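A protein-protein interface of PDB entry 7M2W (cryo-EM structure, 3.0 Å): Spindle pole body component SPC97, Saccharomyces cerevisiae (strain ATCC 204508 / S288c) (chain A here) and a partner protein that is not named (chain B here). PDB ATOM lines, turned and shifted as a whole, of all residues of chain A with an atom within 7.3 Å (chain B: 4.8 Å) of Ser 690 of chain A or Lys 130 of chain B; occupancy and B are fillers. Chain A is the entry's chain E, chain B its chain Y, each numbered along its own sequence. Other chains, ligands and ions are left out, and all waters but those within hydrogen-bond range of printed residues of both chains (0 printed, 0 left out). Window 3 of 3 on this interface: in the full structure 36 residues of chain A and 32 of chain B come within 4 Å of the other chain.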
ATOM      1  N   LEU A 495       6.006  27.597 -13.784  1.00  0.00           N
ATOM      2  CA  LEU A 495       6.513  26.315 -13.304  1.00  0.00           C
ATOM      3  C   LEU A 495       6.669  26.289 -11.790  1.00  0.00           C
ATOM      4  O   LEU A 495       6.609  25.216 -11.180  1.00  0.00           O
ATOM      5  CB  LEU A 495       7.852  26.005 -13.971  1.00  0.00           C
ATOM      6  CG  LEU A 495       7.846  25.528 -15.418  1.00  0.00           C
ATOM      7  CD1 LEU A 495       9.267  25.274 -15.882  1.00  0.00           C
ATOM      8  CD2 LEU A 495       7.033  24.260 -15.505  1.00  0.00           C
ATOM      9  N   TYR A 498       4.237  24.345  -9.512  1.00  0.00           N
ATOM     10  CA  TYR A 498       4.118  22.898  -9.645  1.00  0.00           C
ATOM     11  C   TYR A 498       5.372  22.139  -9.247  1.00  0.00           C
ATOM     12  O   TYR A 498       5.269  21.050  -8.679  1.00  0.00           O
ATOM     13  CB  TYR A 498       3.740  22.541 -11.088  1.00  0.00           C
ATOM     14  CG  TYR A 498       2.650  23.419 -11.653  1.00  0.00           C
ATOM     15  CD1 TYR A 498       2.872  24.202 -12.776  1.00  0.00           C
ATOM     16  CD2 TYR A 498       1.399  23.471 -11.056  1.00  0.00           C
ATOM     17  CE1 TYR A 498       1.875  25.009 -13.290  1.00  0.00           C
ATOM     18  CE2 TYR A 498       0.398  24.273 -11.563  1.00  0.00           C
ATOM     19  CZ  TYR A 498       0.640  25.041 -12.678  1.00  0.00           C
ATOM     20  OH  TYR A 498      -0.358  25.841 -13.185  1.00  0.00           O
ATOM     21  N   LEU A 499       6.552  22.677  -9.524  1.00  0.00           N
ATOM     22  CA  LEU A 499       7.799  21.991  -9.226  1.00  0.00           C
ATOM     23  C   LEU A 499       8.638  22.804  -8.247  1.00  0.00           C
ATOM     24  O   LEU A 499       8.402  23.996  -8.038  1.00  0.00           O
ATOM     25  CB  LEU A 499       8.589  21.728 -10.509  1.00  0.00           C
ATOM     26  CG  LEU A 499       7.908  20.771 -11.493  1.00  0.00           C
ATOM     27  CD1 LEU A 499       7.170  21.540 -12.580  1.00  0.00           C
ATOM     28  CD2 LEU A 499       8.912  19.811 -12.104  1.00  0.00           C
ATOM     29  N   GLN A 500       9.629  22.142  -7.650  1.00  0.00           N
ATOM     30  CA  GLN A 500      10.472  22.753  -6.621  1.00  0.00           C
ATOM     31  C   GLN A 500      11.649  23.468  -7.288  1.00  0.00           C
ATOM     32  O   GLN A 500      12.762  22.950  -7.402  1.00  0.00           O
ATOM     33  CB  GLN A 500      10.947  21.700  -5.629  1.00  0.00           C
ATOM     34  CG  GLN A 500       9.943  21.361  -4.535  1.00  0.00           C
ATOM     35  CD  GLN A 500       8.716  20.634  -5.059  1.00  0.00           C
ATOM     36  OE1 GLN A 500       8.702  20.146  -6.189  1.00  0.00           O
ATOM     37  NE2 GLN A 500       7.677  20.560  -4.235  1.00  0.00           N
ATOM     38  N   ILE A 501      11.377  24.692  -7.743  1.00  0.00           N
ATOM     39  CA  ILE A 501      12.367  25.518  -8.421  1.00  0.00           C
ATOM     40  C   ILE A 501      12.287  26.938  -7.879  1.00  0.00           C
ATOM     41  O   ILE A 501      11.530  27.238  -6.955  1.00  0.00           O
ATOM     42  CB  ILE A 501      12.188  25.527  -9.951  1.00  0.00           C
ATOM     43  CG1 ILE A 501      10.844  26.145 -10.328  1.00  0.00           C
ATOM     44  CG2 ILE A 501      12.292  24.126 -10.509  1.00  0.00           C
ATOM     45  CD1 ILE A 501      10.541  26.040 -11.791  1.00  0.00           C
ATOM     46  N   TYR A 502      13.090  27.817  -8.480  1.00  0.00           N
ATOM     47  CA  TYR A 502      13.176  29.226  -8.146  1.00  0.00           C
ATOM     48  C   TYR A 502      12.967  30.078  -9.396  1.00  0.00           C
ATOM     49  O   TYR A 502      13.345  29.672 -10.501  1.00  0.00           O
ATOM     50  CB  TYR A 502      14.536  29.569  -7.528  1.00  0.00           C
ATOM     51  CG  TYR A 502      14.968  28.637  -6.416  1.00  0.00           C
ATOM     52  CD1 TYR A 502      15.576  27.418  -6.699  1.00  0.00           C
ATOM     53  CD2 TYR A 502      14.770  28.974  -5.083  1.00  0.00           C
ATOM     54  CE1 TYR A 502      15.970  26.564  -5.691  1.00  0.00           C
ATOM     55  CE2 TYR A 502      15.164  28.125  -4.066  1.00  0.00           C
ATOM     56  CZ  TYR A 502      15.763  26.922  -4.376  1.00  0.00           C
ATOM     57  OH  TYR A 502      16.156  26.073  -3.369  1.00  0.00           O
ATOM     58  N   THR A 681       3.252  13.763 -17.420  1.00  0.00           N
ATOM     59  CA  THR A 681       3.892  13.977 -16.127  1.00  0.00           C
ATOM     60  C   THR A 681       5.336  13.490 -16.140  1.00  0.00           C
ATOM     61  O   THR A 681       6.217  14.126 -15.549  1.00  0.00           O
ATOM     62  CB  THR A 681       3.094  13.274 -15.029  1.00  0.00           C
ATOM     63  OG1 THR A 681       1.782  13.844 -14.952  1.00  0.00           O
ATOM     64  CG2 THR A 681       3.779  13.431 -13.686  1.00  0.00           C
ATOM     65  N   ILE A 683       7.045  13.784 -18.662  1.00  0.00           N
ATOM     66  CA  ILE A 683       7.693  14.906 -19.333  1.00  0.00           C
ATOM     67  C   ILE A 683       7.890  16.068 -18.366  1.00  0.00           C
ATOM     68  O   ILE A 683       8.988  16.618 -18.251  1.00  0.00           O
ATOM     69  CB  ILE A 683       6.888  15.342 -20.570  1.00  0.00           C
ATOM     70  CG1 ILE A 683       6.714  14.177 -21.537  1.00  0.00           C
ATOM     71  CG2 ILE A 683       7.602  16.468 -21.276  1.00  0.00           C
ATOM     72  CD1 ILE A 683       5.896  14.516 -22.757  1.00  0.00           C
ATOM     73  N   MET A 684       6.829  16.448 -17.647  1.00  0.00           N
ATOM     74  CA  MET A 684       6.851  17.667 -16.841  1.00  0.00           C
ATOM     75  C   MET A 684       7.881  17.611 -15.720  1.00  0.00           C
ATOM     76  O   MET A 684       8.275  18.655 -15.192  1.00  0.00           O
ATOM     77  CB  MET A 684       5.468  17.926 -16.247  1.00  0.00           C
ATOM     78  CG  MET A 684       4.454  18.513 -17.209  1.00  0.00           C
ATOM     79  SD  MET A 684       4.735  20.255 -17.538  1.00  0.00           S
ATOM     80  CE  MET A 684       5.133  20.857 -15.902  1.00  0.00           C
ATOM     81  N   THR A 685       8.320  16.418 -15.336  1.00  0.00           N
ATOM     82  CA  THR A 685       9.233  16.266 -14.213  1.00  0.00           C
ATOM     83  C   THR A 685      10.591  15.716 -14.623  1.00  0.00           C
ATOM     84  O   THR A 685      11.293  15.141 -13.786  1.00  0.00           O
ATOM     85  CB  THR A 685       8.608  15.368 -13.145  1.00  0.00           C
ATOM     86  OG1 THR A 685       8.220  14.121 -13.731  1.00  0.00           O
ATOM     87  CG2 THR A 685       7.386  16.040 -12.543  1.00  0.00           C
ATOM     88  N   ASN A 686      10.971  15.871 -15.886  1.00  0.00           N
ATOM     89  CA  ASN A 686      12.323  15.538 -16.304  1.00  0.00           C
ATOM     90  C   ASN A 686      13.276  16.667 -15.921  1.00  0.00           C
ATOM     91  O   ASN A 686      12.868  17.820 -15.757  1.00  0.00           O
ATOM     92  CB  ASN A 686      12.365  15.280 -17.810  1.00  0.00           C
ATOM     93  CG  ASN A 686      13.747  14.923 -18.302  1.00  0.00           C
ATOM     94  OD1 ASN A 686      14.370  15.681 -19.045  1.00  0.00           O
ATOM     95  ND2 ASN A 686      14.244  13.766 -17.882  1.00  0.00           N
ATOM     96  N   ARG A 687      14.556  16.314 -15.754  1.00  0.00           N
ATOM     97  CA  ARG A 687      15.564  17.275 -15.312  1.00  0.00           C
ATOM     98  C   ARG A 687      15.535  18.568 -16.117  1.00  0.00           C
ATOM     99  O   ARG A 687      15.630  19.657 -15.541  1.00  0.00           O
ATOM    100  CB  ARG A 687      16.955  16.645 -15.388  1.00  0.00           C
ATOM    101  CG  ARG A 687      17.041  15.277 -14.742  1.00  0.00           C
ATOM    102  CD  ARG A 687      17.525  15.364 -13.304  1.00  0.00           C
ATOM    103  NE  ARG A 687      17.617  14.041 -12.692  1.00  0.00           N
ATOM    104  CZ  ARG A 687      17.757  13.827 -11.388  1.00  0.00           C
ATOM    105  NH1 ARG A 687      17.814  14.851 -10.548  1.00  0.00           N
ATOM    106  NH2 ARG A 687      17.832  12.589 -10.921  1.00  0.00           N
ATOM    107  N   CYS A 688      15.407  18.475 -17.444  1.00  0.00           N
ATOM    108  CA  CYS A 688      15.344  19.673 -18.275  1.00  0.00           C
ATOM    109  C   CYS A 688      14.161  20.569 -17.935  1.00  0.00           C
ATOM    110  O   CYS A 688      14.131  21.723 -18.373  1.00  0.00           O
ATOM    111  CB  CYS A 688      15.286  19.293 -19.754  1.00  0.00           C
ATOM    112  SG  CYS A 688      16.727  18.393 -20.345  1.00  0.00           S
ATOM    113  N   LEU A 689      13.188  20.068 -17.178  1.00  0.00           N
ATOM    114  CA  LEU A 689      12.081  20.884 -16.698  1.00  0.00           C
ATOM    115  C   LEU A 689      12.042  21.015 -15.185  1.00  0.00           C
ATOM    116  O   LEU A 689      11.491  21.997 -14.674  1.00  0.00           O
ATOM    117  CB  LEU A 689      10.748  20.307 -17.180  1.00  0.00           C
ATOM    118  CG  LEU A 689      10.417  20.492 -18.656  1.00  0.00           C
ATOM    119  CD1 LEU A 689       9.242  19.638 -19.029  1.00  0.00           C
ATOM    120  CD2 LEU A 689      10.085  21.943 -18.914  1.00  0.00           C
ATOM    121  N   SER A 690      12.596  20.052 -14.453  1.00  0.00           N
ATOM    122  CA  SER A 690      12.558  20.114 -12.998  1.00  0.00           C
ATOM    123  C   SER A 690      13.830  20.706 -12.398  1.00  0.00           C
ATOM    124  O   SER A 690      13.779  21.732 -11.716  1.00  0.00           O
ATOM    125  CB  SER A 690      12.317  18.716 -12.423  1.00  0.00           C
ATOM    126  OG  SER A 690      13.423  17.866 -12.669  1.00  0.00           O
ATOM    127  N   ASP A 691      14.976  20.079 -12.649  1.00  0.00           N
ATOM    128  CA  ASP A 691      16.186  20.386 -11.897  1.00  0.00           C
ATOM    129  C   ASP A 691      16.991  21.547 -12.458  1.00  0.00           C
ATOM    130  O   ASP A 691      17.682  22.227 -11.692  1.00  0.00           O
ATOM    131  CB  ASP A 691      17.086  19.149 -11.824  1.00  0.00           C
ATOM    132  CG  ASP A 691      18.031  19.188 -10.642  1.00  0.00           C
ATOM    133  OD1 ASP A 691      19.192  18.750 -10.789  1.00  0.00           O
ATOM    134  OD2 ASP A 691      17.612  19.655  -9.564  1.00  0.00           O
ATOM    135  N   LEU A 692      16.928  21.796 -13.762  1.00  0.00           N
ATOM    136  CA  LEU A 692      17.881  22.679 -14.420  1.00  0.00           C
ATOM    137  C   LEU A 692      17.243  23.903 -15.060  1.00  0.00           C
ATOM    138  O   LEU A 692      17.905  24.580 -15.852  1.00  0.00           O
ATOM    139  CB  LEU A 692      18.664  21.895 -15.475  1.00  0.00           C
ATOM    140  CG  LEU A 692      19.428  20.689 -14.928  1.00  0.00           C
ATOM    141  CD1 LEU A 692      20.365  20.130 -15.970  1.00  0.00           C
ATOM    142  CD2 LEU A 692      20.198  21.068 -13.675  1.00  0.00           C
ATOM    143  N   ILE A 693      15.981  24.200 -14.751  1.00  0.00           N
ATOM    144  CA  ILE A 693      15.320  25.353 -15.366  1.00  0.00           C
ATOM    145  C   ILE A 693      16.052  26.666 -15.095  1.00  0.00           C
ATOM    146  O   ILE A 693      16.241  27.442 -16.040  1.00  0.00           O
ATOM    147  CB  ILE A 693      13.839  25.396 -14.961  1.00  0.00           C
ATOM    148  CG1 ILE A 693      13.016  24.505 -15.889  1.00  0.00           C
ATOM    149  CG2 ILE A 693      13.312  26.822 -14.995  1.00  0.00           C
ATOM    150  CD1 ILE A 693      12.884  25.052 -17.295  1.00  0.00           C
ATOM    151  N   PRO A 694      16.478  26.982 -13.865  1.00  0.00           N
ATOM    152  CA  PRO A 694      17.207  28.249 -13.670  1.00  0.00           C
ATOM    153  C   PRO A 694      18.519  28.337 -14.441  1.00  0.00           C
ATOM    154  O   PRO A 694      18.812  29.387 -15.028  1.00  0.00           O
ATOM    155  CB  PRO A 694      17.431  28.287 -12.153  1.00  0.00           C
ATOM    156  CG  PRO A 694      16.328  27.461 -11.599  1.00  0.00           C
ATOM    157  CD  PRO A 694      16.181  26.335 -12.574  1.00  0.00           C
ATOM    158  N   GLN A 696      19.251  26.708 -17.225  1.00  0.00           N
ATOM    159  CA  GLN A 696      18.868  26.868 -18.621  1.00  0.00           C
ATOM    160  C   GLN A 696      18.437  28.294 -18.918  1.00  0.00           C
ATOM    161  O   GLN A 696      18.756  28.820 -19.985  1.00  0.00           O
ATOM    162  CB  GLN A 696      17.756  25.884 -18.985  1.00  0.00           C
ATOM    163  CG  GLN A 696      18.207  24.438 -19.042  1.00  0.00           C
ATOM    164  CD  GLN A 696      17.078  23.492 -19.383  1.00  0.00           C
ATOM    165  OE1 GLN A 696      15.927  23.905 -19.504  1.00  0.00           O
ATOM    166  NE2 GLN A 696      17.400  22.215 -19.542  1.00  0.00           N
ATOM    167  N   GLU B 126      10.289   7.080  -4.545  1.00  0.00           N
ATOM    168  CA  GLU B 126      10.738   8.475  -4.656  1.00  0.00           C
ATOM    169  C   GLU B 126      10.296   9.095  -5.989  1.00  0.00           C
ATOM    170  O   GLU B 126       9.727  10.185  -6.015  1.00  0.00           O
ATOM    171  CB  GLU B 126      12.270   8.544  -4.530  1.00  0.00           C
ATOM    172  CG  GLU B 126      12.812   8.154  -3.146  1.00  0.00           C
ATOM    173  CD  GLU B 126      12.768   9.259  -2.090  1.00  0.00           C
ATOM    174  OE1 GLU B 126      12.168  10.330  -2.309  1.00  0.00           O
ATOM    175  OE2 GLU B 126      13.344   9.036  -1.015  1.00  0.00           O
ATOM    176  N   HIS B 127      10.480   8.372  -7.097  1.00  0.00           N
ATOM    177  CA  HIS B 127      10.058   8.809  -8.427  1.00  0.00           C
ATOM    178  C   HIS B 127       8.530   8.958  -8.537  1.00  0.00           C
ATOM    179  O   HIS B 127       8.041   9.993  -8.989  1.00  0.00           O
ATOM    180  CB  HIS B 127      10.644   7.820  -9.444  1.00  0.00           C
ATOM    181  CG  HIS B 127      10.365   8.142 -10.886  1.00  0.00           C
ATOM    182  ND1 HIS B 127      10.761   9.268 -11.566  1.00  0.00           N
ATOM    183  CD2 HIS B 127       9.720   7.338 -11.782  1.00  0.00           C
ATOM    184  CE1 HIS B 127      10.380   9.143 -12.845  1.00  0.00           C
ATOM    185  NE2 HIS B 127       9.734   7.980 -13.026  1.00  0.00           N
ATOM    186  N   GLN B 128       7.749   7.989  -8.052  1.00  0.00           N
ATOM    187  CA  GLN B 128       6.286   8.089  -8.018  1.00  0.00           C
ATOM    188  C   GLN B 128       5.799   9.227  -7.110  1.00  0.00           C
ATOM    189  O   GLN B 128       4.919   9.984  -7.507  1.00  0.00           O
ATOM    190  CB  GLN B 128       5.661   6.752  -7.597  1.00  0.00           C
ATOM    191  CG  GLN B 128       5.790   5.681  -8.687  1.00  0.00           C
ATOM    192  CD  GLN B 128       5.127   4.355  -8.332  1.00  0.00           C
ATOM    193  OE1 GLN B 128       4.529   4.169  -7.291  1.00  0.00           O
ATOM    194  NE2 GLN B 128       5.197   3.377  -9.192  1.00  0.00           N
ATOM    195  N   MET B 129       6.400   9.427  -5.935  1.00  0.00           N
ATOM    196  CA  MET B 129       6.052  10.541  -5.046  1.00  0.00           C
ATOM    197  C   MET B 129       6.373  11.906  -5.669  1.00  0.00           C
ATOM    198  O   MET B 129       5.606  12.847  -5.485  1.00  0.00           O
ATOM    199  CB  MET B 129       6.716  10.378  -3.675  1.00  0.00           C
ATOM    200  CG  MET B 129       6.045   9.266  -2.863  1.00  0.00           C
ATOM    201  SD  MET B 129       6.606   9.108  -1.148  1.00  0.00           S
ATOM    202  CE  MET B 129       8.292   8.530  -1.382  1.00  0.00           C
ATOM    203  N   LYS B 130       7.428  12.022  -6.483  1.00  0.00           N
ATOM    204  CA  LYS B 130       7.716  13.241  -7.256  1.00  0.00           C
ATOM    205  C   LYS B 130       6.593  13.571  -8.249  1.00  0.00           C
ATOM    206  O   LYS B 130       6.113  14.702  -8.281  1.00  0.00           O
ATOM    207  CB  LYS B 130       9.089  13.089  -7.929  1.00  0.00           C
ATOM    208  CG  LYS B 130       9.628  14.414  -8.476  1.00  0.00           C
ATOM    209  CD  LYS B 130      11.072  14.246  -8.957  1.00  0.00           C
ATOM    210  CE  LYS B 130      11.687  15.590  -9.332  1.00  0.00           C
ATOM    211  NZ  LYS B 130      13.119  15.466  -9.663  1.00  0.00           N
ATOM    212  N   LYS B 131       6.104  12.573  -8.994  1.00  0.00           N
ATOM    213  CA  LYS B 131       4.930  12.709  -9.884  1.00  0.00           C
ATOM    214  C   LYS B 131       3.666  13.077  -9.105  1.00  0.00           C
ATOM    215  O   LYS B 131       2.934  13.973  -9.512  1.00  0.00           O
ATOM    216  CB  LYS B 131       4.685  11.414 -10.677  1.00  0.00           C
ATOM    217  CG  LYS B 131       5.858  11.010 -11.573  1.00  0.00           C
ATOM    218  CD  LYS B 131       5.542   9.717 -12.328  1.00  0.00           C
ATOM    219  CE  LYS B 131       6.820   9.143 -12.925  1.00  0.00           C
ATOM    220  NZ  LYS B 131       6.576   7.918 -13.717  1.00  0.00           N
ATOM    221  N   GLU B 132       3.441  12.421  -7.971  1.00  0.00           N
ATOM    222  CA  GLU B 132       2.288  12.652  -7.098  1.00  0.00           C
ATOM    223  C   GLU B 132       2.244  14.098  -6.590  1.00  0.00           C
ATOM    224  O   GLU B 132       1.245  14.783  -6.793  1.00  0.00           O
ATOM    225  CB  GLU B 132       2.335  11.643  -5.938  1.00  0.00           C
ATOM    226  CG  GLU B 132       1.115  11.667  -5.013  1.00  0.00           C
ATOM    227  CD  GLU B 132      -0.154  11.042  -5.609  1.00  0.00           C
ATOM    228  OE1 GLU B 132      -0.146  10.588  -6.772  1.00  0.00           O
ATOM    229  OE2 GLU B 132      -1.171  11.001  -4.881  1.00  0.00           O
ATOM    230  N   ARG B 133       3.337  14.602  -6.000  1.00  0.00           N
ATOM    231  CA  ARG B 133       3.424  15.987  -5.507  1.00  0.00           C
ATOM    232  C   ARG B 133       3.132  17.000  -6.611  1.00  0.00           C
ATOM    233  O   ARG B 133       2.335  17.910  -6.405  1.00  0.00           O
ATOM    234  CB  ARG B 133       4.805  16.256  -4.889  1.00  0.00           C
ATOM    235  CG  ARG B 133       4.990  15.579  -3.526  1.00  0.00           C
ATOM    236  CD  ARG B 133       6.283  16.016  -2.837  1.00  0.00           C
ATOM    237  NE  ARG B 133       7.493  15.618  -3.578  1.00  0.00           N
ATOM    238  CZ  ARG B 133       8.285  14.596  -3.331  1.00  0.00           C
ATOM    239  NH1 ARG B 133       8.030  13.727  -2.410  1.00  0.00           N
ATOM    240  NH2 ARG B 133       9.372  14.431  -4.013  1.00  0.00           N
ATOM    241  N   PHE B 134       3.708  16.805  -7.794  1.00  0.00           N
ATOM    242  CA  PHE B 134       3.441  17.642  -8.962  1.00  0.00           C
ATOM    243  C   PHE B 134       1.956  17.631  -9.375  1.00  0.00           C
ATOM    244  O   PHE B 134       1.334  18.687  -9.484  1.00  0.00           O
ATOM    245  CB  PHE B 134       4.354  17.202 -10.115  1.00  0.00           C
ATOM    246  CG  PHE B 134       3.862  17.667 -11.463  1.00  0.00           C
ATOM    247  CD1 PHE B 134       3.957  19.017 -11.814  1.00  0.00           C
ATOM    248  CD2 PHE B 134       3.174  16.779 -12.301  1.00  0.00           C
ATOM    249  CE1 PHE B 134       3.346  19.480 -12.986  1.00  0.00           C
ATOM    250  CE2 PHE B 134       2.602  17.230 -13.497  1.00  0.00           C
ATOM    251  CZ  PHE B 134       2.675  18.589 -13.832  1.00  0.00           C
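Phe 134 of chain B touches Tyr 498 of chain A.
CG2 of Thr 681 of chain A touches CB of Lys 131 of chain B, 3.7 Å away.
Thr 681 of chain A touches Phe 134 of chain B (CG2 to CD2, 3.7 Å).
CE1 of Phe 134 of chain B touches CE of Met 684 of chain A (3.7 Å).
OG of Ser 690 of chain A touches NZ of Lys 130 of chain B (3.9 Å).
Lys 130 of chain B touches one residue of chain A.
Of the printed residues of chain A, Lys 131 of chain B touches Thr 681.
Of the printed residues of chain A, Phe 134 of chain B touches Tyr 498 (3.6 Å), Thr 681 (3.7 Å) and Met 684 (3.7 Å).
Of the printed residues of chain B, Met 684 of chain A touches Phe 134 (3.7 Å).
Arg 133 of chain B touches none of the printed residues of chain A.
The nearest printed residue of chain B that does not touch Ser 690 of chain A is Phe 134 of chain B (8.4 Å).
The nearest printed residue of chain B that does not touch Met 684 of chain A is Lys 130 of chain B (7.4 Å).
A ring nitrogen (NE2) of His 127 of chain B sits close to the side-chain amino group (NZ) of Lys 131 of chain B, 3.2 Å away.
The backbone carbonyl oxygen (O) of Asn 686 of chain A sits at hydrogen-bond distance from the side-chain hydroxyl (OG) of Ser 690 of chain A, at 3.1 Å.
The backbone carbonyl oxygen (O) of Thr 681 of chain A lies within hydrogen-bond range of the side-chain hydroxyl (OG1) of Thr 685 of chain A, 2.7 Å away.
Hydrophobic or aromatic side chains of chain B within 4 Å of the printed part of chain A: Phe 134.
Of the 20 printed residues of chain A, 4 touch a printed residue of chain B.
Printed residues of chain A that touch a printed residue of chain B: Tyr 498, Thr 681, Met 684 and Ser 690.
Along chain A the printed residues that touch a printed residue of chain B span positions 498 to 690.
Among the printed residues, no Asp or Glu carboxylate lies within 4 Å of a Lys or Arg side-chain nitrogen of the other chain.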
